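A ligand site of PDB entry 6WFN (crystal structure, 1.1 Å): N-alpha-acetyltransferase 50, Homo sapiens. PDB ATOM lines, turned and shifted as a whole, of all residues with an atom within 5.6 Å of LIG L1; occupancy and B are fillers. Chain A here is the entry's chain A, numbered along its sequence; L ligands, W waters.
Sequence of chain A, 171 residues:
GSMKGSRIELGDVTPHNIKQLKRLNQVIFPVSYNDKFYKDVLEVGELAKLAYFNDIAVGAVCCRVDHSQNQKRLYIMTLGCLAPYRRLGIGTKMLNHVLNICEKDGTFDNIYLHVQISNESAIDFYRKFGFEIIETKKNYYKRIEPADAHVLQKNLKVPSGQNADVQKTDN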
ATOM      1  N   PHE A  29     -10.701  -7.143   1.997  1.00  0.00           N
ATOM      2  CA  PHE A  29     -10.138  -7.365   3.329  1.00  0.00           C
ATOM      3  C   PHE A  29     -11.135  -7.928   4.322  1.00  0.00           C
ATOM      4  O   PHE A  29     -12.341  -7.674   4.179  1.00  0.00           O
ATOM      5  CB  PHE A  29      -9.514  -6.052   3.861  1.00  0.00           C
ATOM      6  CG  PHE A  29      -8.407  -5.556   2.950  1.00  0.00           C
ATOM      7  CD1 PHE A  29      -7.165  -6.193   2.922  1.00  0.00           C
ATOM      8  CD2 PHE A  29      -8.623  -4.506   2.092  1.00  0.00           C
ATOM      9  CE1 PHE A  29      -6.167  -5.749   2.031  1.00  0.00           C
ATOM     10  CE2 PHE A  29      -7.639  -4.110   1.177  1.00  0.00           C
ATOM     11  CZ  PHE A  29      -6.427  -4.745   1.160  1.00  0.00           C
ATOM     12  N   PRO A  30     -10.636  -8.656   5.326  1.00  0.00           N
ATOM     13  CA  PRO A  30     -11.536  -9.307   6.290  1.00  0.00           C
ATOM     14  C   PRO A  30     -11.991  -8.408   7.436  1.00  0.00           C
ATOM     15  O   PRO A  30     -12.773  -8.862   8.299  1.00  0.00           O
ATOM     16  CB  PRO A  30     -10.689 -10.461   6.796  1.00  0.00           C
ATOM     17  CG  PRO A  30      -9.278  -9.936   6.757  1.00  0.00           C
ATOM     18  CD  PRO A  30      -9.235  -9.103   5.521  1.00  0.00           C
ATOM     19  N   VAL A  31     -11.459  -7.176   7.528  1.00  0.00           N
ATOM     20  CA  VAL A  31     -11.830  -6.219   8.558  1.00  0.00           C
ATOM     21  C   VAL A  31     -12.378  -4.998   7.870  1.00  0.00           C
ATOM     22  O   VAL A  31     -12.061  -4.710   6.705  1.00  0.00           O
ATOM     23  CB  VAL A  31     -10.651  -5.848   9.485  1.00  0.00           C
ATOM     24  CG1 VAL A  31     -10.141  -7.082  10.244  1.00  0.00           C
ATOM     25  CG2 VAL A  31      -9.500  -5.170   8.707  1.00  0.00           C
ATOM     26  N   SER A  32     -13.205  -4.256   8.592  1.00  0.00           N
ATOM     27  CA  SER A  32     -13.763  -3.032   8.049  1.00  0.00           C
ATOM     28  C   SER A  32     -12.887  -1.829   8.381  1.00  0.00           C
ATOM     29  O   SER A  32     -12.183  -1.829   9.392  1.00  0.00           O
ATOM     30  CB  SER A  32     -15.176  -2.805   8.601  1.00  0.00           C
ATOM     31  OG  SER A  32     -15.120  -2.688  10.009  1.00  0.00           O
ATOM     32  N   TYR A  33     -12.927  -0.819   7.537  1.00  0.00           N
ATOM     33  CA  TYR A  33     -12.223   0.435   7.768  1.00  0.00           C
ATOM     34  C   TYR A  33     -13.256   1.509   7.959  1.00  0.00           C
ATOM     35  O   TYR A  33     -14.263   1.547   7.252  1.00  0.00           O
ATOM     36  CB  TYR A  33     -11.238   0.758   6.622  1.00  0.00           C
ATOM     37  CG  TYR A  33     -10.091  -0.233   6.617  1.00  0.00           C
ATOM     38  CD1 TYR A  33      -8.988  -0.048   7.460  1.00  0.00           C
ATOM     39  CD2 TYR A  33     -10.190  -1.441   5.941  1.00  0.00           C
ATOM     40  CE1 TYR A  33      -7.981  -1.002   7.536  1.00  0.00           C
ATOM     41  CE2 TYR A  33      -9.215  -2.422   6.045  1.00  0.00           C
ATOM     42  CZ  TYR A  33      -8.132  -2.199   6.874  1.00  0.00           C
ATOM     43  OH  TYR A  33      -7.152  -3.127   7.024  1.00  0.00           O
ATOM     44  N   PHE A  37     -10.634   6.543   8.193  1.00  0.00           N
ATOM     45  CA  PHE A  37      -9.667   5.963   7.262  1.00  0.00           C
ATOM     46  C   PHE A  37      -9.840   6.582   5.869  1.00  0.00           C
ATOM     47  O   PHE A  37      -8.861   7.002   5.225  1.00  0.00           O
ATOM     48  CB  PHE A  37      -9.825   4.440   7.238  1.00  0.00           C
ATOM     49  CG  PHE A  37      -8.963   3.782   6.191  1.00  0.00           C
ATOM     50  CD1 PHE A  37      -7.670   3.379   6.490  1.00  0.00           C
ATOM     51  CD2 PHE A  37      -9.451   3.559   4.921  1.00  0.00           C
ATOM     52  CE1 PHE A  37      -6.885   2.714   5.533  1.00  0.00           C
ATOM     53  CE2 PHE A  37      -8.655   2.932   3.953  1.00  0.00           C
ATOM     54  CZ  PHE A  37      -7.386   2.510   4.271  1.00  0.00           C
ATOM     55  N   ASP A  40      -8.744  10.184   5.655  1.00  0.00           N
ATOM     56  CA  ASP A  40      -7.308  10.311   5.683  1.00  0.00           C
ATOM     57  C   ASP A  40      -6.664   9.970   4.344  1.00  0.00           C
ATOM     58  O   ASP A  40      -5.690  10.593   3.951  1.00  0.00           O
ATOM     59  CB  ASP A  40      -6.710   9.466   6.825  1.00  0.00           C
ATOM     60  CG  ASP A  40      -7.135   9.959   8.195  1.00  0.00           C
ATOM     61  OD1 ASP A  40      -7.676  11.074   8.279  1.00  0.00           O
ATOM     62  OD2 ASP A  40      -6.983   9.196   9.178  1.00  0.00           O
ATOM     63  N   ARG A  64       0.395   5.821   4.517  1.00  0.00           N
ATOM     64  CA  ARG A  64       0.591   7.094   5.174  1.00  0.00           C
ATOM     65  C   ARG A  64       2.016   7.214   5.656  1.00  0.00           C
ATOM     66  O   ARG A  64       2.721   6.217   5.798  1.00  0.00           O
ATOM     67  CB  ARG A  64      -0.413   7.325   6.307  1.00  0.00           C
ATOM     68  CG  ARG A  64      -0.176   6.416   7.503  1.00  0.00           C
ATOM     69  CD  ARG A  64      -1.176   6.598   8.659  1.00  0.00           C
ATOM     70  NE  ARG A  64      -1.256   8.009   9.067  1.00  0.00           N
ATOM     71  CZ  ARG A  64      -0.386   8.626   9.877  1.00  0.00           C
ATOM     72  NH1 ARG A  64       0.553   7.940  10.502  1.00  0.00           N
ATOM     73  NH2 ARG A  64      -0.484   9.932  10.087  1.00  0.00           N
ATOM     74  N   TYR A  75       4.047   3.684   6.118  1.00  0.00           N
ATOM     75  CA  TYR A  75       3.196   2.627   6.624  1.00  0.00           C
ATOM     76  C   TYR A  75       2.169   2.263   5.553  1.00  0.00           C
ATOM     77  O   TYR A  75       1.355   3.110   5.164  1.00  0.00           O
ATOM     78  CB  TYR A  75       2.508   3.088   7.918  1.00  0.00           C
ATOM     79  CG  TYR A  75       1.662   1.994   8.540  1.00  0.00           C
ATOM     80  CD1 TYR A  75       2.219   0.768   8.876  1.00  0.00           C
ATOM     81  CD2 TYR A  75       0.328   2.207   8.846  1.00  0.00           C
ATOM     82  CE1 TYR A  75       1.455  -0.259   9.447  1.00  0.00           C
ATOM     83  CE2 TYR A  75      -0.439   1.209   9.444  1.00  0.00           C
ATOM     84  CZ  TYR A  75       0.122  -0.025   9.730  1.00  0.00           C
ATOM     85  OH  TYR A  75      -0.653  -1.011  10.285  1.00  0.00           O
ATOM     86  N   ILE A  76       2.207   1.027   5.054  1.00  0.00           N
ATOM     87  CA  ILE A  76       1.224   0.538   4.093  1.00  0.00           C
ATOM     88  C   ILE A  76       0.044   0.007   4.887  1.00  0.00           C
ATOM     89  O   ILE A  76       0.208  -1.011   5.586  1.00  0.00           O
ATOM     90  CB  ILE A  76       1.804  -0.534   3.178  1.00  0.00           C
ATOM     91  CG1 ILE A  76       3.068  -0.069   2.434  1.00  0.00           C
ATOM     92  CG2 ILE A  76       0.709  -0.962   2.185  1.00  0.00           C
ATOM     93  CD1 ILE A  76       3.707  -1.140   1.568  1.00  0.00           C
ATOM     94  N   MET A  77      -1.103   0.653   4.808  1.00  0.00           N
ATOM     95  CA  MET A  77      -2.269   0.217   5.558  1.00  0.00           C
ATOM     96  C   MET A  77      -3.038  -0.881   4.853  1.00  0.00           C
ATOM     97  O   MET A  77      -3.407  -1.890   5.468  1.00  0.00           O
ATOM     98  CB  MET A  77      -3.193   1.412   5.819  1.00  0.00           C
ATOM     99  CG  MET A  77      -2.563   2.436   6.727  1.00  0.00           C
ATOM    100  SD  MET A  77      -3.529   3.907   7.039  1.00  0.00           S
ATOM    101  CE  MET A  77      -3.378   4.692   5.432  1.00  0.00           C
ATOM    102  N   THR A  78      -3.268  -0.699   3.549  1.00  0.00           N
ATOM    103  CA  THR A  78      -4.007  -1.663   2.759  1.00  0.00           C
ATOM    104  C   THR A  78      -3.370  -1.761   1.375  1.00  0.00           C
ATOM    105  O   THR A  78      -2.990  -0.726   0.808  1.00  0.00           O
ATOM    106  CB  THR A  78      -5.514  -1.338   2.645  1.00  0.00           C
ATOM    107  OG1 THR A  78      -5.713  -0.047   2.104  1.00  0.00           O
ATOM    108  CG2 THR A  78      -6.244  -1.422   3.968  1.00  0.00           C
ATOM    109  N   HIS A 114       1.443  -4.362   8.593  1.00  0.00           N
ATOM    110  CA  HIS A 114       0.992  -5.492   9.378  1.00  0.00           C
ATOM    111  C   HIS A 114       0.302  -6.486   8.461  1.00  0.00           C
ATOM    112  O   HIS A 114      -0.429  -6.097   7.556  1.00  0.00           O
ATOM    113  CB  HIS A 114      -0.024  -5.027  10.431  1.00  0.00           C
ATOM    114  CG  HIS A 114       0.596  -4.280  11.553  1.00  0.00           C
ATOM    115  ND1 HIS A 114       0.687  -2.897  11.545  1.00  0.00           N
ATOM    116  CD2 HIS A 114       1.101  -4.732  12.716  1.00  0.00           C
ATOM    117  CE1 HIS A 114       1.273  -2.563  12.672  1.00  0.00           C
ATOM    118  NE2 HIS A 114       1.578  -3.643  13.391  1.00  0.00           N
ATOM    119  N   VAL A 115       0.502  -7.772   8.744  1.00  0.00           N
ATOM    120  CA  VAL A 115      -0.182  -8.809   8.009  1.00  0.00           C
ATOM    121  C   VAL A 115      -0.546  -9.958   8.925  1.00  0.00           C
ATOM    122  O   VAL A 115       0.280 -10.454   9.689  1.00  0.00           O
ATOM    123  CB  VAL A 115       0.602  -9.281   6.781  1.00  0.00           C
ATOM    124  CG1 VAL A 115       1.945  -9.858   7.156  1.00  0.00           C
ATOM    125  CG2 VAL A 115      -0.190 -10.274   5.943  1.00  0.00           C
ATOM    126  N   GLN A 116      -1.775 -10.382   8.810  1.00  0.00           N
ATOM    127  CA  GLN A 116      -2.278 -11.525   9.574  1.00  0.00           C
ATOM    128  C   GLN A 116      -1.342 -12.717   9.326  1.00  0.00           C
ATOM    129  O   GLN A 116      -0.959 -12.993   8.190  1.00  0.00           O
ATOM    130  CB  GLN A 116      -3.695 -11.809   9.110  1.00  0.00           C
ATOM    131  CG  GLN A 116      -4.465 -12.708  10.030  1.00  0.00           C
ATOM    132  CD  GLN A 116      -5.860 -12.946   9.503  1.00  0.00           C
ATOM    133  OE1 GLN A 116      -6.180 -12.685   8.328  1.00  0.00           O
ATOM    134  NE2 GLN A 116      -6.708 -13.465  10.387  1.00  0.00           N
ATOM    135  N   ASN A 119      -1.720 -15.304   6.423  1.00  0.00           N
ATOM    136  CA  ASN A 119      -1.700 -14.910   5.026  1.00  0.00           C
ATOM    137  C   ASN A 119      -0.341 -15.166   4.412  1.00  0.00           C
ATOM    138  O   ASN A 119       0.440 -14.255   4.119  1.00  0.00           O
ATOM    139  CB  ASN A 119      -2.123 -13.456   4.942  1.00  0.00           C
ATOM    140  CG  ASN A 119      -2.518 -13.046   3.566  1.00  0.00           C
ATOM    141  OD1 ASN A 119      -2.180 -13.682   2.568  1.00  0.00           O
ATOM    142  ND2 ASN A 119      -3.261 -11.940   3.464  1.00  0.00           N
ATOM    143  N   TYR A 140      -3.346  -8.351  17.568  1.00  0.00           N
ATOM    144  CA  TYR A 140      -3.391  -7.128  16.788  1.00  0.00           C
ATOM    145  C   TYR A 140      -4.791  -6.992  16.222  1.00  0.00           C
ATOM    146  O   TYR A 140      -5.389  -5.921  16.274  1.00  0.00           O
ATOM    147  CB  TYR A 140      -2.333  -7.209  15.674  1.00  0.00           C
ATOM    148  CG  TYR A 140      -2.354  -5.971  14.805  1.00  0.00           C
ATOM    149  CD1 TYR A 140      -1.730  -4.800  15.210  1.00  0.00           C
ATOM    150  CD2 TYR A 140      -3.081  -5.939  13.622  1.00  0.00           C
ATOM    151  CE1 TYR A 140      -1.759  -3.654  14.427  1.00  0.00           C
ATOM    152  CE2 TYR A 140      -3.132  -4.791  12.835  1.00  0.00           C
ATOM    153  CZ  TYR A 140      -2.509  -3.642  13.263  1.00  0.00           C
ATOM    154  OH  TYR A 140      -2.594  -2.531  12.469  1.00  0.00           O
ATOM    155  N   TYR A 141      -5.332  -8.084  15.664  1.00  0.00           N
ATOM    156  CA  TYR A 141      -6.694  -8.024  15.169  1.00  0.00           C
ATOM    157  C   TYR A 141      -7.642  -8.390  16.291  1.00  0.00           C
ATOM    158  O   TYR A 141      -7.313  -9.189  17.167  1.00  0.00           O
ATOM    159  CB  TYR A 141      -6.908  -8.937  13.966  1.00  0.00           C
ATOM    160  CG  TYR A 141      -5.968  -8.588  12.831  1.00  0.00           C
ATOM    161  CD1 TYR A 141      -6.199  -7.466  12.042  1.00  0.00           C
ATOM    162  CD2 TYR A 141      -4.853  -9.370  12.580  1.00  0.00           C
ATOM    163  CE1 TYR A 141      -5.297  -7.091  11.040  1.00  0.00           C
ATOM    164  CE2 TYR A 141      -3.944  -9.016  11.586  1.00  0.00           C
ATOM    165  CZ  TYR A 141      -4.167  -7.861  10.836  1.00  0.00           C
ATOM    166  OH  TYR A 141      -3.207  -7.551   9.909  1.00  0.00           O
ATOM    167  N   LYS A 142      -8.800  -7.802  16.261  1.00  0.00           N
ATOM    168  CA  LYS A 142      -9.724  -8.061  17.359  1.00  0.00           C
ATOM    169  C   LYS A 142     -10.872  -8.977  17.002  1.00  0.00           C
ATOM    170  O   LYS A 142     -11.318  -9.733  17.881  1.00  0.00           O
ATOM    171  CB  LYS A 142     -10.225  -6.730  17.938  1.00  0.00           C
ATOM    172  CG  LYS A 142      -9.127  -5.696  18.265  1.00  0.00           C
ATOM    173  CD  LYS A 142      -8.027  -6.167  19.233  1.00  0.00           C
ATOM    174  CE  LYS A 142      -6.947  -5.122  19.397  1.00  0.00           C
ATOM    175  NZ  LYS A 142      -5.967  -5.508  20.440  1.00  0.00           N
ATOM    176  N   ARG A 143     -11.361  -8.946  15.751  1.00  0.00           N
ATOM    177  CA  ARG A 143     -12.535  -9.724  15.359  1.00  0.00           C
ATOM    178  C   ARG A 143     -12.287 -10.900  14.425  1.00  0.00           C
ATOM    179  O   ARG A 143     -13.229 -11.630  14.134  1.00  0.00           O
ATOM    180  CB  ARG A 143     -13.585  -8.815  14.733  1.00  0.00           C
ATOM    181  CG  ARG A 143     -14.063  -7.684  15.652  1.00  0.00           C
ATOM    182  CD  ARG A 143     -15.044  -6.778  14.931  1.00  0.00           C
ATOM    183  N   ILE A 144     -11.049 -11.076  13.951  1.00  0.00           N
ATOM    184  CA  ILE A 144     -10.719 -12.154  13.020  1.00  0.00           C
ATOM    185  C   ILE A 144      -9.746 -13.102  13.624  1.00  0.00           C
ATOM    186  O   ILE A 144      -9.028 -12.747  14.558  1.00  0.00           O
ATOM    187  CB  ILE A 144     -10.238 -11.619  11.658  1.00  0.00           C
ATOM    188  CG1 ILE A 144      -8.923 -10.812  11.792  1.00  0.00           C
ATOM    189  CG2 ILE A 144     -11.350 -10.822  10.941  1.00  0.00           C
ATOM    190  CD1 ILE A 144      -8.197 -10.432  10.456  1.00  0.00           C
HETATM  191  C1  LIG L   1      -8.802  -3.146  11.883  1.00  0.00           C
HETATM  192  C2  LIG L   1      -7.534  -3.975  13.704  1.00  0.00           C
HETATM  193  C3  LIG L   1      -7.802  -2.244  11.590  1.00  0.00           C
HETATM  194  C4  LIG L   1      -6.535  -3.051  13.430  1.00  0.00           C
HETATM  195  C5  LIG L   1      -5.893   3.140   9.967  1.00  0.00           C
HETATM  196  C6  LIG L   1      -8.667  -4.011  12.948  1.00  0.00           C
HETATM  197  C7  LIG L   1      -6.677  -2.202  12.368  1.00  0.00           C
HETATM  198  C8  LIG L   1      -4.626   3.306  10.502  1.00  0.00           C
HETATM  199  C9  LIG L   1      -9.751  -4.989  13.258  1.00  0.00           C
HETATM  200  C10 LIG L   1      -4.593   1.101  10.277  1.00  0.00           C
HETATM  201  C11 LIG L   1      -5.829  -6.036   6.447  1.00  0.00           C
HETATM  202  C12 LIG L   1      -3.939  -7.487   6.922  1.00  0.00           C
HETATM  203  C13 LIG L   1      -5.604  -1.227  12.045  1.00  0.00           C
HETATM  204  C14 LIG L   1      -4.071   4.604  10.837  1.00  0.00           C
HETATM  205  C15 LIG L   1      -3.627  -4.454   8.007  1.00  0.00           C
HETATM  206  C16 LIG L   1      -4.848  -5.039   5.899  1.00  0.00           C
HETATM  207  C17 LIG L   1      -3.623  -0.861   9.019  1.00  0.00           C
HETATM  208  C18 LIG L   1      -5.032  -2.496   9.992  1.00  0.00           C
HETATM  209  C19 LIG L   1      -4.102  -0.295  10.348  1.00  0.00           C
HETATM  210  C20 LIG L   1      -3.518  -5.069   6.625  1.00  0.00           C
HETATM  211  C21 LIG L   1      -3.718  -2.353   9.249  1.00  0.00           C
HETATM  212  C22 LIG L   1      -6.204  -8.237   7.416  1.00  0.00           C
HETATM  213  C23 LIG L   1      -2.398   5.818  12.131  1.00  0.00           C
HETATM  214  N1  LIG L   1      -9.571  -6.110  13.983  1.00  0.00           N
HETATM  215  N2  LIG L   1      -3.909   2.147  10.690  1.00  0.00           N
HETATM  216  N3  LIG L   1     -10.986  -4.826  12.796  1.00  0.00           N
HETATM  217  N4  LIG L   1     -10.800  -6.705  13.966  1.00  0.00           N
HETATM  218  N5  LIG L   1     -11.637  -5.926  13.262  1.00  0.00           N
HETATM  219  N6  LIG L   1      -3.078  -6.438   6.737  1.00  0.00           N
HETATM  220  N7  LIG L   1      -5.286  -7.179   6.944  1.00  0.00           N
HETATM  221  N8  LIG L   1      -5.107  -1.273  10.770  1.00  0.00           N
HETATM  222  N9  LIG L   1      -2.892   4.603  11.503  1.00  0.00           N
HETATM  223  N10 LIG L   1      -3.666  -3.092   7.998  1.00  0.00           N
HETATM  224  O1  LIG L   1      -7.046  -5.830   6.430  1.00  0.00           O
HETATM  225  O2  LIG L   1      -3.510  -8.624   7.091  1.00  0.00           O
HETATM  226  O3  LIG L   1      -5.256  -0.365  12.839  1.00  0.00           O
HETATM  227  O4  LIG L   1      -4.689   5.621  10.545  1.00  0.00           O
HETATM  228  O5  LIG L   1      -3.689  -5.088   9.054  1.00  0.00           O
HETATM  229  S1  LIG L   1      -6.170   1.473   9.705  1.00  0.00           S
HETATM  230  N1  LG2 L   2       0.986 -17.703  -4.763  1.00  0.00           N
HETATM  231  C1  LG2 L   2       2.245 -17.728  -5.223  1.00  0.00           C
HETATM  232  N2  LG2 L   2       3.003 -16.704  -5.641  1.00  0.00           N
HETATM  233  C2  LG2 L   2       2.324 -15.541  -5.577  1.00  0.00           C
HETATM  234  C3  LG2 L   2       1.017 -15.368  -5.150  1.00  0.00           C
HETATM  235  C4  LG2 L   2       0.333 -16.520  -4.704  1.00  0.00           C
HETATM  236  N3  LG2 L   2      -0.895 -16.492  -4.171  1.00  0.00           N
HETATM  237  N4  LG2 L   2       0.653 -14.031  -5.221  1.00  0.00           N
HETATM  238  C5  LG2 L   2       1.740 -13.434  -5.649  1.00  0.00           C
HETATM  239  N5  LG2 L   2       2.790 -14.281  -5.879  1.00  0.00           N
HETATM  240  C6  LG2 L   2       4.162 -13.900  -6.239  1.00  0.00           C
HETATM  241  C7  LG2 L   2       4.617 -14.422  -7.590  1.00  0.00           C
HETATM  242  O1  LG2 L   2       6.021 -14.629  -7.570  1.00  0.00           O
HETATM  243  C8  LG2 L   2       4.227 -13.260  -8.481  1.00  0.00           C
HETATM  244  O2  LG2 L   2       4.974 -13.190  -9.713  1.00  0.00           O
HETATM  245  P1  LG2 L   2       4.700 -14.203 -10.915  1.00  0.00           P
HETATM  246  O3  LG2 L   2       5.369 -13.618 -12.064  1.00  0.00           O
HETATM  247  O4  LG2 L   2       5.154 -15.608 -10.495  1.00  0.00           O
HETATM  248  O5  LG2 L   2       3.258 -14.257 -11.083  1.00  0.00           O
HETATM  249  C9  LG2 L   2       4.592 -12.058  -7.627  1.00  0.00           C
HETATM  250  O6  LG2 L   2       4.269 -12.478  -6.287  1.00  0.00           O
HETATM  251  C10 LG2 L   2       3.839 -10.789  -7.968  1.00  0.00           C
HETATM  252  O7  LG2 L   2       2.434 -11.059  -7.926  1.00  0.00           O
HETATM  253  P2  LG2 L   2       1.377 -10.011  -8.467  1.00  0.00           P
HETATM  254  O8  LG2 L   2       0.676 -10.560  -9.635  1.00  0.00           O
HETATM  255  O9  LG2 L   2       1.996  -8.646  -8.633  1.00  0.00           O
HETATM  256  O10 LG2 L   2       0.436  -9.963  -7.188  1.00  0.00           O
HETATM  257  P3  LG2 L   2      -1.132  -9.730  -7.087  1.00  0.00           P
HETATM  258  O11 LG2 L   2      -1.573  -8.669  -8.051  1.00  0.00           O
HETATM  259  O12 LG2 L   2      -1.831 -11.058  -7.192  1.00  0.00           O
HETATM  260  O13 LG2 L   2      -1.244  -9.150  -5.652  1.00  0.00           O
HETATM  261  C11 LG2 L   2      -1.704  -9.614  -3.309  1.00  0.00           C
HETATM  262  C12 LG2 L   2      -0.760  -9.838  -4.484  1.00  0.00           C
HETATM  263  C13 LG2 L   2      -1.882  -8.095  -3.117  1.00  0.00           C
HETATM  264  C14 LG2 L   2      -1.068 -10.229  -2.060  1.00  0.00           C
HETATM  265  C15 LG2 L   2      -3.058 -10.305  -3.603  1.00  0.00           C
HETATM  266  O14 LG2 L   2      -2.895 -11.729  -3.485  1.00  0.00           O
HETATM  267  C16 LG2 L   2      -4.230  -9.868  -2.727  1.00  0.00           C
HETATM  268  O15 LG2 L   2      -4.845  -8.841  -2.984  1.00  0.00           O
HETATM  269  N6  LG2 L   2      -4.481 -10.631  -1.673  1.00  0.00           N
HETATM  270  C17 LG2 L   2      -5.580 -10.357  -0.760  1.00  0.00           C
HETATM  271  C18 LG2 L   2      -5.347  -9.127   0.082  1.00  0.00           C
HETATM  272  C19 LG2 L   2      -3.995  -9.169   0.734  1.00  0.00           C
HETATM  273  O16 LG2 L   2      -3.537 -10.216   1.222  1.00  0.00           O
HETATM  274  N7  LG2 L   2      -3.310  -8.029   0.747  1.00  0.00           N
HETATM  275  C20 LG2 L   2      -2.077  -7.848   1.486  1.00  0.00           C
HETATM  276  C21 LG2 L   2      -2.399  -7.792   2.973  1.00  0.00           C
HETATM  277  S1  LG2 L   2      -1.109  -6.868   3.854  1.00  0.00           S
HETATM  278  C22 LG2 L   2      -1.698  -5.227   3.565  1.00  0.00           C
HETATM  279  O17 LG2 L   2      -2.765  -4.998   3.074  1.00  0.00           O
HETATM  280  C23 LG2 L   2      -0.791  -4.162   4.109  1.00  0.00           C
HETATM  281  O   HOH W   1      -0.809   3.170  12.852  1.00  0.00           O
HETATM  282  O   HOH W   2     -12.509  -2.674  12.000  1.00  0.00           O
HETATM  283  O   HOH W   3      -0.590  -2.560   7.692  1.00  0.00           O
HETATM  284  O   HOH W   4      -7.066   6.521   9.488  1.00  0.00           O
HETATM  285  O   HOH W   5      -4.593 -10.866   5.814  1.00  0.00           O
HETATM  286  O   HOH W   6      -4.911   8.008  11.685  1.00  0.00           O
HETATM  287  O   HOH W   7     -13.913  -5.721  11.267  1.00  0.00           O
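The side-chain hydroxyl of Tyr 141 is in hydrogen-bond range of an oxygen (O5) of LIG L1.
An oxygen (O1) of LIG L1 sits at hydrogen-bond distance from the side-chain hydroxyl of Tyr 33, 2.8 Å away.
O of His 114 is in hydrogen-bond range of N6 of LIG L1, 2.8 Å away.
A nitrogen (N10) of LIG L1 sits at hydrogen-bond distance from the backbone carbonyl oxygen (O) of Met 77 (2.8 Å).
The backbone NH (N) of Arg 143 sits at hydrogen-bond distance from a nitrogen (N4) of LIG L1.
N1 of LIG L1 lies within hydrogen-bond range of N of Lys 142 (2.9 Å).
The backbone NH of Gln 116 is in hydrogen-bond range of an oxygen (O2) of LIG L1, 3.0 Å away.
OH of Tyr 140 sits close to O3 of LIG L1 (3.5 Å).
An oxygen (O16) of LG2 L2 sits at hydrogen-bond distance from the side-chain amide nitrogen (ND2) of Asn 119.
A nitrogen (N6) of LIG L1 sits close to a sulfur (S1) of LG2 L2 (3.5 Å).
OH of Tyr 141 lies within hydrogen-bond range of N of Gln 116 (3.4 Å).
ND1 of His 114 sits at hydrogen-bond distance from OH of Tyr 75, at 2.6 Å.
A ring nitrogen (ND1) of His 114 is in hydrogen-bond range of the side-chain hydroxyl (OH) of Tyr 140 (3.4 Å).
The side-chain hydroxyl (OH) of Tyr 75 is in hydrogen-bond range of the side-chain hydroxyl (OH) of Tyr 140.
N of Tyr 75 is in hydrogen-bond range of O of Arg 64 (2.9 Å).
Merely in contact with LIG L1: Phe 29, Pro 30, Val 31, Phe 37, Arg 64, Tyr 75 and Val 115.
Hydrophobic or aromatic side chains that line LIG L1: Phe 29, Pro 30, Val 31, Tyr 33, Phe 37, Tyr 75, Met 77, His 114, Val 115, Tyr 140 and Tyr 141.
15 residues have an atom within 4 Å of LIG L1: Phe 29, Pro 30, Val 31, Tyr 33, Phe 37, Arg 64, Tyr 75, Met 77, His 114, Val 115, Gln 116, Tyr 140, Tyr 141, Lys 142 and Arg 143.
Water W6 lies within hydrogen-bond range of an oxygen (O4) of LIG L1 (2.7 Å) and the side-chain carboxylate of Asp 40 (3.5 Å).
Water W4 lies within hydrogen-bond range of the side-chain carboxylate of Asp 40 (2.7 Å) and an oxygen (O4) of LIG L1 (2.8 Å).
Water W2 bridges a nitrogen (N3) of LIG L1 (2.8 Å) and the backbone carbonyl oxygen of Ser 32 (2.8 Å).
Water W5 lies within hydrogen-bond range of O2 of LIG L1, ND2 of Asn 119 and OE1 of Gln 116.
Water W7 lies within hydrogen-bond range of a nitrogen (N5) of LIG L1 (3.0 Å) and the backbone NH of Ser 32 (3.1 Å).
Water W3 lies within hydrogen-bond range of the backbone carbonyl oxygen (O) of Ile 76 (2.7 Å), the backbone NH (N) of His 114 (2.9 Å), the side-chain hydroxyl (OH) of Tyr 75 (3.0 Å) and a nitrogen (N10) of LIG L1 (3.1 Å).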
